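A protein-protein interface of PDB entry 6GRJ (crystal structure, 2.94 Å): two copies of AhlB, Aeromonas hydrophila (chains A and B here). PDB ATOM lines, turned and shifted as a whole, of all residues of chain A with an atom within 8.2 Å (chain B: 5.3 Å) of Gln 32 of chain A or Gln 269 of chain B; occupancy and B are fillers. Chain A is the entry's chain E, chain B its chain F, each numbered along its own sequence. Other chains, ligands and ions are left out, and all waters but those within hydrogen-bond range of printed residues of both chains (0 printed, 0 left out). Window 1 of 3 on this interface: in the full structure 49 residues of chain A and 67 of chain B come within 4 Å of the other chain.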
ATOM      1  N   GLN A  24      23.763   3.830 -17.457  1.00  0.00           N
ATOM      2  CA  GLN A  24      24.050   2.409 -17.347  1.00  0.00           C
ATOM      3  C   GLN A  24      22.742   1.673 -17.014  1.00  0.00           C
ATOM      4  O   GLN A  24      22.356   0.674 -17.671  1.00  0.00           O
ATOM      5  CB  GLN A  24      25.113   2.187 -16.286  1.00  0.00           C
ATOM      6  CG  GLN A  24      25.656   0.769 -16.269  1.00  0.00           C
ATOM      7  CD  GLN A  24      26.811   0.639 -15.312  1.00  0.00           C
ATOM      8  OE1 GLN A  24      27.748  -0.111 -15.563  1.00  0.00           O
ATOM      9  NE2 GLN A  24      26.746   1.334 -14.178  1.00  0.00           N
ATOM     10  N   THR A  25      22.033   2.202 -16.011  1.00  0.00           N
ATOM     11  CA  THR A  25      20.803   1.593 -15.582  1.00  0.00           C
ATOM     12  C   THR A  25      19.777   1.581 -16.713  1.00  0.00           C
ATOM     13  O   THR A  25      19.062   0.597 -16.924  1.00  0.00           O
ATOM     14  CB  THR A  25      20.154   2.361 -14.440  1.00  0.00           C
ATOM     15  OG1 THR A  25      21.099   2.426 -13.372  1.00  0.00           O
ATOM     16  CG2 THR A  25      18.855   1.725 -13.990  1.00  0.00           C
ATOM     17  N   TYR A  26      19.656   2.718 -17.390  1.00  0.00           N
ATOM     18  CA  TYR A  26      18.683   2.856 -18.458  1.00  0.00           C
ATOM     19  C   TYR A  26      19.026   1.843 -19.553  1.00  0.00           C
ATOM     20  O   TYR A  26      18.156   1.215 -20.089  1.00  0.00           O
ATOM     21  CB  TYR A  26      18.595   4.301 -18.965  1.00  0.00           C
ATOM     22  CG  TYR A  26      17.221   4.643 -19.459  1.00  0.00           C
ATOM     23  CD1 TYR A  26      16.802   4.300 -20.728  1.00  0.00           C
ATOM     24  CD2 TYR A  26      16.299   5.230 -18.616  1.00  0.00           C
ATOM     25  CE1 TYR A  26      15.510   4.574 -21.169  1.00  0.00           C
ATOM     26  CE2 TYR A  26      15.006   5.505 -19.029  1.00  0.00           C
ATOM     27  CZ  TYR A  26      14.607   5.172 -20.309  1.00  0.00           C
ATOM     28  OH  TYR A  26      13.331   5.443 -20.704  1.00  0.00           O
ATOM     29  N   CYS A  27      20.306   1.651 -19.852  1.00  0.00           N
ATOM     30  CA  CYS A  27      20.707   0.731 -20.913  1.00  0.00           C
ATOM     31  C   CYS A  27      20.365  -0.708 -20.517  1.00  0.00           C
ATOM     32  O   CYS A  27      19.841  -1.441 -21.333  1.00  0.00           O
ATOM     33  CB  CYS A  27      22.174   0.909 -21.232  1.00  0.00           C
ATOM     34  SG  CYS A  27      22.543   2.465 -22.057  1.00  0.00           S
ATOM     35  N   ASN A  28      20.660  -1.112 -19.280  1.00  0.00           N
ATOM     36  CA  ASN A  28      20.305  -2.463 -18.801  1.00  0.00           C
ATOM     37  C   ASN A  28      18.776  -2.634 -18.865  1.00  0.00           C
ATOM     38  O   ASN A  28      18.231  -3.668 -19.202  1.00  0.00           O
ATOM     39  CB  ASN A  28      20.862  -2.726 -17.404  1.00  0.00           C
ATOM     40  CG  ASN A  28      22.337  -3.039 -17.420  1.00  0.00           C
ATOM     41  OD1 ASN A  28      22.834  -3.662 -18.353  1.00  0.00           O
ATOM     42  ND2 ASN A  28      23.023  -2.698 -16.346  1.00  0.00           N
ATOM     43  N   SER A  29      18.077  -1.561 -18.546  1.00  0.00           N
ATOM     44  CA  SER A  29      16.657  -1.563 -18.561  1.00  0.00           C
ATOM     45  C   SER A  29      16.108  -1.682 -20.008  1.00  0.00           C
ATOM     46  O   SER A  29      15.172  -2.358 -20.285  1.00  0.00           O
ATOM     47  CB  SER A  29      16.185  -0.361 -17.806  1.00  0.00           C
ATOM     48  OG  SER A  29      14.778  -0.305 -17.859  1.00  0.00           O
ATOM     49  N   VAL A  30      16.713  -0.996 -20.951  1.00  0.00           N
ATOM     50  CA  VAL A  30      16.288  -1.011 -22.365  1.00  0.00           C
ATOM     51  C   VAL A  30      16.539  -2.403 -22.952  1.00  0.00           C
ATOM     52  O   VAL A  30      15.748  -2.877 -23.720  1.00  0.00           O
ATOM     53  CB  VAL A  30      16.983   0.071 -23.223  1.00  0.00           C
ATOM     54  CG1 VAL A  30      16.806  -0.146 -24.717  1.00  0.00           C
ATOM     55  CG2 VAL A  30      16.537   1.467 -22.861  1.00  0.00           C
ATOM     56  N   LYS A  31      17.647  -3.033 -22.589  1.00  0.00           N
ATOM     57  CA  LYS A  31      18.044  -4.331 -23.147  1.00  0.00           C
ATOM     58  C   LYS A  31      17.063  -5.427 -22.703  1.00  0.00           C
ATOM     59  O   LYS A  31      16.926  -6.455 -23.346  1.00  0.00           O
ATOM     60  CB  LYS A  31      19.473  -4.676 -22.741  1.00  0.00           C
ATOM     61  CG  LYS A  31      20.560  -3.966 -23.549  1.00  0.00           C
ATOM     62  CD  LYS A  31      21.906  -4.653 -23.527  1.00  0.00           C
ATOM     63  CE  LYS A  31      21.819  -5.956 -24.295  1.00  0.00           C
ATOM     64  NZ  LYS A  31      22.892  -6.906 -23.937  1.00  0.00           N
ATOM     65  N   GLN A  32      16.337  -5.187 -21.619  1.00  0.00           N
ATOM     66  CA  GLN A  32      15.419  -6.141 -21.019  1.00  0.00           C
ATOM     67  C   GLN A  32      14.035  -6.077 -21.684  1.00  0.00           C
ATOM     68  O   GLN A  32      13.209  -6.919 -21.418  1.00  0.00           O
ATOM     69  CB  GLN A  32      15.377  -5.870 -19.522  1.00  0.00           C
ATOM     70  CG  GLN A  32      16.705  -6.179 -18.849  1.00  0.00           C
ATOM     71  CD  GLN A  32      16.655  -6.146 -17.341  1.00  0.00           C
ATOM     72  OE1 GLN A  32      15.792  -6.775 -16.734  1.00  0.00           O
ATOM     73  NE2 GLN A  32      17.610  -5.464 -16.702  1.00  0.00           N
ATOM     74  N   GLN A  33      13.771  -5.054 -22.495  1.00  0.00           N
ATOM     75  CA  GLN A  33      12.460  -4.834 -23.122  1.00  0.00           C
ATOM     76  C   GLN A  33      12.022  -6.033 -23.964  1.00  0.00           C
ATOM     77  O   GLN A  33      12.838  -6.749 -24.466  1.00  0.00           O
ATOM     78  CB  GLN A  33      12.440  -3.588 -23.997  1.00  0.00           C
ATOM     79  CG  GLN A  33      12.603  -2.327 -23.171  1.00  0.00           C
ATOM     80  CD  GLN A  33      11.844  -1.193 -23.804  1.00  0.00           C
ATOM     81  OE1 GLN A  33      10.629  -1.306 -23.930  1.00  0.00           O
ATOM     82  NE2 GLN A  33      12.530  -0.114 -24.184  1.00  0.00           N
ATOM     83  N   VAL A  34      10.712  -6.112 -24.173  1.00  0.00           N
ATOM     84  CA  VAL A  34      10.070  -7.211 -24.801  1.00  0.00           C
ATOM     85  C   VAL A  34       9.544  -6.807 -26.173  1.00  0.00           C
ATOM     86  O   VAL A  34       8.885  -5.784 -26.310  1.00  0.00           O
ATOM     87  CB  VAL A  34       8.886  -7.641 -23.925  1.00  0.00           C
ATOM     88  CG1 VAL A  34       7.989  -8.667 -24.631  1.00  0.00           C
ATOM     89  CG2 VAL A  34       9.320  -8.119 -22.557  1.00  0.00           C
ATOM     90  N   PRO A  35       9.745  -7.631 -27.212  1.00  0.00           N
ATOM     91  CA  PRO A  35       9.214  -7.326 -28.533  1.00  0.00           C
ATOM     92  C   PRO A  35       7.686  -7.405 -28.529  1.00  0.00           C
ATOM     93  O   PRO A  35       7.092  -7.969 -27.592  1.00  0.00           O
ATOM     94  CB  PRO A  35       9.806  -8.441 -29.405  1.00  0.00           C
ATOM     95  CG  PRO A  35      10.881  -9.089 -28.580  1.00  0.00           C
ATOM     96  CD  PRO A  35      10.448  -8.919 -27.162  1.00  0.00           C
ATOM     97  N   LEU A  55      13.366  -1.711 -31.919  1.00  0.00           N
ATOM     98  CA  LEU A  55      13.777  -2.125 -30.574  1.00  0.00           C
ATOM     99  C   LEU A  55      15.192  -2.714 -30.623  1.00  0.00           C
ATOM    100  O   LEU A  55      16.054  -2.388 -29.817  1.00  0.00           O
ATOM    101  CB  LEU A  55      12.781  -3.151 -30.046  1.00  0.00           C
ATOM    102  CG  LEU A  55      13.173  -3.820 -28.730  1.00  0.00           C
ATOM    103  CD1 LEU A  55      13.397  -2.792 -27.640  1.00  0.00           C
ATOM    104  CD2 LEU A  55      12.163  -4.864 -28.312  1.00  0.00           C
ATOM    105  N   LYS A  59      18.586  -1.556 -28.592  1.00  0.00           N
ATOM    106  CA  LYS A  59      19.374  -2.433 -27.734  1.00  0.00           C
ATOM    107  C   LYS A  59      20.840  -2.361 -28.180  1.00  0.00           C
ATOM    108  O   LYS A  59      21.761  -2.405 -27.383  1.00  0.00           O
ATOM    109  CB  LYS A  59      18.813  -3.851 -27.753  1.00  0.00           C
ATOM    110  CG  LYS A  59      17.389  -3.973 -27.239  1.00  0.00           C
ATOM    111  CD  LYS A  59      16.980  -5.357 -26.898  1.00  0.00           C
ATOM    112  CE  LYS A  59      15.633  -5.413 -26.211  1.00  0.00           C
ATOM    113  NZ  LYS A  59      15.242  -6.791 -25.842  1.00  0.00           N
ATOM    114  N   ALA A  62      22.244   0.636 -26.653  1.00  0.00           N
ATOM    115  CA  ALA A  62      22.489   0.367 -25.240  1.00  0.00           C
ATOM    116  C   ALA A  62      23.804  -0.410 -25.067  1.00  0.00           C
ATOM    117  O   ALA A  62      24.586  -0.076 -24.210  1.00  0.00           O
ATOM    118  CB  ALA A  62      21.320  -0.385 -24.673  1.00  0.00           C
ATOM    119  N   GLN A 260       5.464   1.756 -24.993  1.00  0.00           N
ATOM    120  CA  GLN A 260       6.493   1.677 -23.977  1.00  0.00           C
ATOM    121  C   GLN A 260       7.863   1.677 -24.643  1.00  0.00           C
ATOM    122  O   GLN A 260       8.708   2.254 -24.142  1.00  0.00           O
ATOM    123  CB  GLN A 260       6.278   0.431 -23.129  1.00  0.00           C
ATOM    124  CG  GLN A 260       7.184   0.276 -21.915  1.00  0.00           C
ATOM    125  CD  GLN A 260       6.871  -1.022 -21.211  1.00  0.00           C
ATOM    126  OE1 GLN A 260       7.751  -1.835 -20.913  1.00  0.00           O
ATOM    127  NE2 GLN A 260       5.583  -1.255 -20.991  1.00  0.00           N
ATOM    128  N   ILE B 136      20.137 -10.756 -18.832  1.00  0.00           N
ATOM    129  CA  ILE B 136      19.246  -9.801 -19.483  1.00  0.00           C
ATOM    130  C   ILE B 136      18.236 -10.579 -20.327  1.00  0.00           C
ATOM    131  O   ILE B 136      17.084 -10.233 -20.327  1.00  0.00           O
ATOM    132  CB  ILE B 136      20.074  -8.785 -20.292  1.00  0.00           C
ATOM    133  CG1 ILE B 136      20.703  -7.770 -19.334  1.00  0.00           C
ATOM    134  CG2 ILE B 136      19.206  -8.101 -21.331  1.00  0.00           C
ATOM    135  CD1 ILE B 136      21.642  -6.779 -19.989  1.00  0.00           C
ATOM    136  N   SER B 139      15.807 -12.340 -17.833  1.00  0.00           N
ATOM    137  CA  SER B 139      14.938 -11.322 -17.259  1.00  0.00           C
ATOM    138  C   SER B 139      13.846 -10.912 -18.269  1.00  0.00           C
ATOM    139  O   SER B 139      12.678 -10.816 -17.923  1.00  0.00           O
ATOM    140  CB  SER B 139      15.720 -10.129 -16.798  1.00  0.00           C
ATOM    141  OG  SER B 139      14.850  -9.040 -16.522  1.00  0.00           O
ATOM    142  N   SER B 140      14.250 -10.708 -19.524  1.00  0.00           N
ATOM    143  CA  SER B 140      13.348 -10.291 -20.577  1.00  0.00           C
ATOM    144  C   SER B 140      12.318 -11.373 -20.877  1.00  0.00           C
ATOM    145  O   SER B 140      11.151 -11.055 -20.981  1.00  0.00           O
ATOM    146  CB  SER B 140      14.094  -9.943 -21.839  1.00  0.00           C
ATOM    147  OG  SER B 140      13.198  -9.520 -22.859  1.00  0.00           O
ATOM    148  N   PHE B 142      11.219 -13.610 -19.039  1.00  0.00           N
ATOM    149  CA  PHE B 142      10.308 -13.733 -17.931  1.00  0.00           C
ATOM    150  C   PHE B 142       9.252 -12.614 -17.959  1.00  0.00           C
ATOM    151  O   PHE B 142       8.029 -12.886 -17.792  1.00  0.00           O
ATOM    152  CB  PHE B 142      11.079 -13.798 -16.612  1.00  0.00           C
ATOM    153  CG  PHE B 142      11.994 -14.981 -16.439  1.00  0.00           C
ATOM    154  CD1 PHE B 142      11.747 -16.188 -17.074  1.00  0.00           C
ATOM    155  CD2 PHE B 142      13.070 -14.901 -15.580  1.00  0.00           C
ATOM    156  CE1 PHE B 142      12.593 -17.265 -16.900  1.00  0.00           C
ATOM    157  CE2 PHE B 142      13.914 -15.986 -15.395  1.00  0.00           C
ATOM    158  CZ  PHE B 142      13.672 -17.168 -16.052  1.00  0.00           C
ATOM    159  N   GLN B 143       9.706 -11.372 -18.188  1.00  0.00           N
ATOM    160  CA  GLN B 143       8.798 -10.217 -18.264  1.00  0.00           C
ATOM    161  C   GLN B 143       7.726 -10.540 -19.320  1.00  0.00           C
ATOM    162  O   GLN B 143       6.527 -10.288 -19.118  1.00  0.00           O
ATOM    163  CB  GLN B 143       9.602  -8.945 -18.582  1.00  0.00           C
ATOM    164  CG  GLN B 143       8.802  -7.654 -18.575  1.00  0.00           C
ATOM    165  CD  GLN B 143       8.017  -7.499 -17.289  1.00  0.00           C
ATOM    166  OE1 GLN B 143       8.465  -7.860 -16.184  1.00  0.00           O
ATOM    167  NE2 GLN B 143       6.821  -6.945 -17.429  1.00  0.00           N
ATOM    168  N   GLY B 264       4.797 -16.480 -10.097  1.00  0.00           N
ATOM    169  CA  GLY B 264       6.074 -17.178 -10.072  1.00  0.00           C
ATOM    170  C   GLY B 264       7.113 -16.501 -10.959  1.00  0.00           C
ATOM    171  O   GLY B 264       8.266 -16.208 -10.544  1.00  0.00           O
ATOM    172  N   TYR B 265       6.698 -16.256 -12.204  1.00  0.00           N
ATOM    173  CA  TYR B 265       7.580 -15.629 -13.200  1.00  0.00           C
ATOM    174  C   TYR B 265       7.832 -14.177 -12.789  1.00  0.00           C
ATOM    175  O   TYR B 265       8.966 -13.773 -12.968  1.00  0.00           O
ATOM    176  CB  TYR B 265       7.193 -15.979 -14.644  1.00  0.00           C
ATOM    177  CG  TYR B 265       7.653 -17.375 -14.982  1.00  0.00           C
ATOM    178  CD1 TYR B 265       8.964 -17.617 -15.356  1.00  0.00           C
ATOM    179  CD2 TYR B 265       6.821 -18.471 -14.819  1.00  0.00           C
ATOM    180  CE1 TYR B 265       9.417 -18.906 -15.617  1.00  0.00           C
ATOM    181  CE2 TYR B 265       7.257 -19.760 -15.070  1.00  0.00           C
ATOM    182  CZ  TYR B 265       8.561 -19.978 -15.466  1.00  0.00           C
ATOM    183  OH  TYR B 265       9.007 -21.244 -15.681  1.00  0.00           O
ATOM    184  N   LYS B 266       6.865 -13.433 -12.212  1.00  0.00           N
ATOM    185  CA  LYS B 266       7.142 -12.080 -11.741  1.00  0.00           C
ATOM    186  C   LYS B 266       8.312 -12.105 -10.755  1.00  0.00           C
ATOM    187  O   LYS B 266       9.195 -11.251 -10.807  1.00  0.00           O
ATOM    188  CB  LYS B 266       5.953 -11.430 -11.031  1.00  0.00           C
ATOM    189  CG  LYS B 266       4.933 -10.778 -11.947  1.00  0.00           C
ATOM    190  CD  LYS B 266       3.704 -10.256 -11.177  1.00  0.00           C
ATOM    191  CE  LYS B 266       2.740  -9.498 -12.062  1.00  0.00           C
ATOM    192  NZ  LYS B 266       1.325  -9.657 -11.625  1.00  0.00           N
ATOM    193  N   GLY B 267       8.306 -13.099  -9.874  1.00  0.00           N
ATOM    194  CA  GLY B 267       9.331 -13.215  -8.870  1.00  0.00           C
ATOM    195  C   GLY B 267      10.691 -13.531  -9.465  1.00  0.00           C
ATOM    196  O   GLY B 267      11.733 -12.979  -9.042  1.00  0.00           O
ATOM    197  N   LEU B 268      10.670 -14.456 -10.425  1.00  0.00           N
ATOM    198  CA  LEU B 268      11.879 -14.866 -11.104  1.00  0.00           C
ATOM    199  C   LEU B 268      12.467 -13.669 -11.841  1.00  0.00           C
ATOM    200  O   LEU B 268      13.686 -13.450 -11.785  1.00  0.00           O
ATOM    201  CB  LEU B 268      11.551 -16.012 -12.063  1.00  0.00           C
ATOM    202  CG  LEU B 268      11.633 -17.392 -11.423  1.00  0.00           C
ATOM    203  CD1 LEU B 268      11.185 -18.451 -12.408  1.00  0.00           C
ATOM    204  CD2 LEU B 268      13.039 -17.671 -10.895  1.00  0.00           C
ATOM    205  N   GLN B 269      11.575 -12.906 -12.486  1.00  0.00           N
ATOM    206  CA  GLN B 269      11.917 -11.692 -13.235  1.00  0.00           C
ATOM    207  C   GLN B 269      12.691 -10.762 -12.320  1.00  0.00           C
ATOM    208  O   GLN B 269      13.756 -10.287 -12.694  1.00  0.00           O
ATOM    209  CB  GLN B 269      10.666 -10.999 -13.799  1.00  0.00           C
ATOM    210  CG  GLN B 269      10.932  -9.964 -14.879  1.00  0.00           C
ATOM    211  CD  GLN B 269      11.513  -8.698 -14.313  1.00  0.00           C
ATOM    212  OE1 GLN B 269      10.958  -8.080 -13.419  1.00  0.00           O
ATOM    213  NE2 GLN B 269      12.652  -8.296 -14.841  1.00  0.00           N
ATOM    214  N   VAL B 270      12.181 -10.548 -11.101  1.00  0.00           N
ATOM    215  CA  VAL B 270      12.864  -9.683 -10.156  1.00  0.00           C
ATOM    216  C   VAL B 270      14.253 -10.246  -9.845  1.00  0.00           C
ATOM    217  O   VAL B 270      15.241  -9.487  -9.840  1.00  0.00           O
ATOM    218  CB  VAL B 270      12.061  -9.493  -8.860  1.00  0.00           C
ATOM    219  CG1 VAL B 270      12.894  -8.793  -7.802  1.00  0.00           C
ATOM    220  CG2 VAL B 270      10.770  -8.746  -9.092  1.00  0.00           C
ATOM    221  N   GLN B 271      14.332 -11.557  -9.577  1.00  0.00           N
ATOM    222  CA  GLN B 271      15.618 -12.138  -9.208  1.00  0.00           C
ATOM    223  C   GLN B 271      16.632 -11.901 -10.332  1.00  0.00           C
ATOM    224  O   GLN B 271      17.801 -11.570 -10.072  1.00  0.00           O
ATOM    225  CB  GLN B 271      15.480 -13.622  -8.878  1.00  0.00           C
ATOM    226  CG  GLN B 271      14.739 -13.865  -7.563  1.00  0.00           C
ATOM    227  CD  GLN B 271      14.738 -15.318  -7.186  1.00  0.00           C
ATOM    228  OE1 GLN B 271      13.950 -16.114  -7.705  1.00  0.00           O
ATOM    229  NE2 GLN B 271      15.622 -15.666  -6.269  1.00  0.00           N
ATOM    230  N   ALA B 272      16.159 -12.042 -11.573  1.00  0.00           N
ATOM    231  CA  ALA B 272      17.001 -11.909 -12.758  1.00  0.00           C
ATOM    232  C   ALA B 272      17.479 -10.457 -12.915  1.00  0.00           C
ATOM    233  O   ALA B 272      18.649 -10.209 -13.190  1.00  0.00           O
ATOM    234  CB  ALA B 272      16.249 -12.400 -13.972  1.00  0.00           C
ATOM    235  N   GLN B 273      16.560  -9.511 -12.717  1.00  0.00           N
ATOM    236  CA  GLN B 273      16.844  -8.094 -12.813  1.00  0.00           C
ATOM    237  C   GLN B 273      17.911  -7.739 -11.776  1.00  0.00           C
ATOM    238  O   GLN B 273      18.843  -7.006 -12.099  1.00  0.00           O
ATOM    239  CB  GLN B 273      15.532  -7.329 -12.636  1.00  0.00           C
ATOM    240  CG  GLN B 273      15.614  -5.863 -13.051  1.00  0.00           C
ATOM    241  CD  GLN B 273      14.300  -5.404 -13.629  1.00  0.00           C
ATOM    242  OE1 GLN B 273      13.206  -5.809 -13.199  1.00  0.00           O
ATOM    243  NE2 GLN B 273      14.424  -4.589 -14.656  1.00  0.00           N
ATOM    244  N   ASN B 274      17.794  -8.293 -10.564  1.00  0.00           N
ATOM    245  CA  ASN B 274      18.778  -8.056  -9.497  1.00  0.00           C
ATOM    246  C   ASN B 274      20.133  -8.630  -9.904  1.00  0.00           C
ATOM    247  O   ASN B 274      21.175  -8.074  -9.555  1.00  0.00           O
ATOM    248  CB  ASN B 274      18.375  -8.673  -8.159  1.00  0.00           C
ATOM    249  CG  ASN B 274      17.136  -8.043  -7.567  1.00  0.00           C
ATOM    250  OD1 ASN B 274      16.856  -6.869  -7.806  1.00  0.00           O
ATOM    251  ND2 ASN B 274      16.389  -8.819  -6.793  1.00  0.00           N
ATOM    252  N   VAL B 276      21.233  -8.910 -12.987  1.00  0.00           N
ATOM    253  CA  VAL B 276      21.778  -8.036 -14.017  1.00  0.00           C
ATOM    254  C   VAL B 276      22.558  -6.915 -13.330  1.00  0.00           C
ATOM    255  O   VAL B 276      23.684  -6.611 -13.687  1.00  0.00           O
ATOM    256  CB  VAL B 276      20.697  -7.436 -14.928  1.00  0.00           C
ATOM    257  CG1 VAL B 276      21.258  -6.307 -15.775  1.00  0.00           C
ATOM    258  CG2 VAL B 276      20.045  -8.497 -15.803  1.00  0.00           C
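No position is printed for both chains.
Of the 16 printed residues of chain A, 5 touch a printed residue of chain B. Hydrophobic or aromatic side chains of chain A within 4 Å of the printed part of chain B: Val 34. Among the printed residues, 10 pairs touch across the chains. Among the printed residues, no Asp or Glu carboxylate lies within 4 Å of a Lys or Arg side-chain nitrogen of the other chain.
Printed residues of chain B within 4 Å of Gln 32 of chain A: Ser 139 (2.5 Å), Ser 140 (3.0 Å), Gln 269 (3.97 Å), Gln 273 (3.3 Å) and Val 276 (3.9 Å). Of the printed residues of chain A, Ser 139 of chain B touches Gln 32. Of chain A, only Gln 32 (3.97 Å) comes within 4 Å of Gln 269 of chain B. Printed residues of chain A within 4 Å of Gln 273 of chain B: Gln 32. Printed residues of chain A within 4 Å of Val 276 of chain B: Asn 28 and Gln 32. The nearest printed residue of chain A that does not touch Val 276 of chain B is Ser 29 of chain A (6.3 Å).
The backbone carbonyl oxygen (O) of Asn 28 of chain A sits close to the side-chain amide nitrogen (NE2) of Gln 32 of chain A (3.1 Å). NZ of Lys 59 of chain A is in hydrogen-bond range of O of Lys 31 of chain A, 3.0 Å away. The side-chain amino group (NZ) of Lys 59 of chain A sits at hydrogen-bond distance from the backbone carbonyl oxygen (O) of Gln 33 of chain A. The side-chain hydroxyl (OG) of Ser 139 of chain B lies within hydrogen-bond range of the side-chain amide nitrogen (NE2) of Gln 269 of chain B (2.9 Å). The side-chain amide oxygen of Gln 273 of chain B is in hydrogen-bond range of the side-chain amide nitrogen of Gln 269 of chain B, 3.0 Å away.
Among the printed residues, merely in contact across the chains: Lys 31 of chain A with Ile 136 of chain B (3.5 Å), Asn 28 of chain A with Ile 136 of chain B (3.7 Å), Val 34 of chain A with Ser 140 of chain B (3.8 Å), Asn 28 of chain A with Val 276 of chain B (3.8 Å), Gln 32 of chain A with Val 276 of chain B (3.9 Å) and Gln 32 of chain A with Gln 269 of chain B (3.97 Å).
The side-chain amide oxygen of Gln 32 of chain A sits at hydrogen-bond distance from the side-chain hydroxyl of Ser 139 of chain B (2.5 Å). The side-chain hydroxyl (OG) of Ser 140 of chain B lies within hydrogen-bond range of the backbone carbonyl oxygen (O) of Gln 32 of chain A. The side-chain amide oxygen of Gln 32 of chain A is in hydrogen-bond range of the side-chain amide nitrogen of Gln 273 of chain B, 3.3 Å away. O of Gln 33 of chain A sits at hydrogen-bond distance from OG of Ser 140 of chain B, at 3.2 Å.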
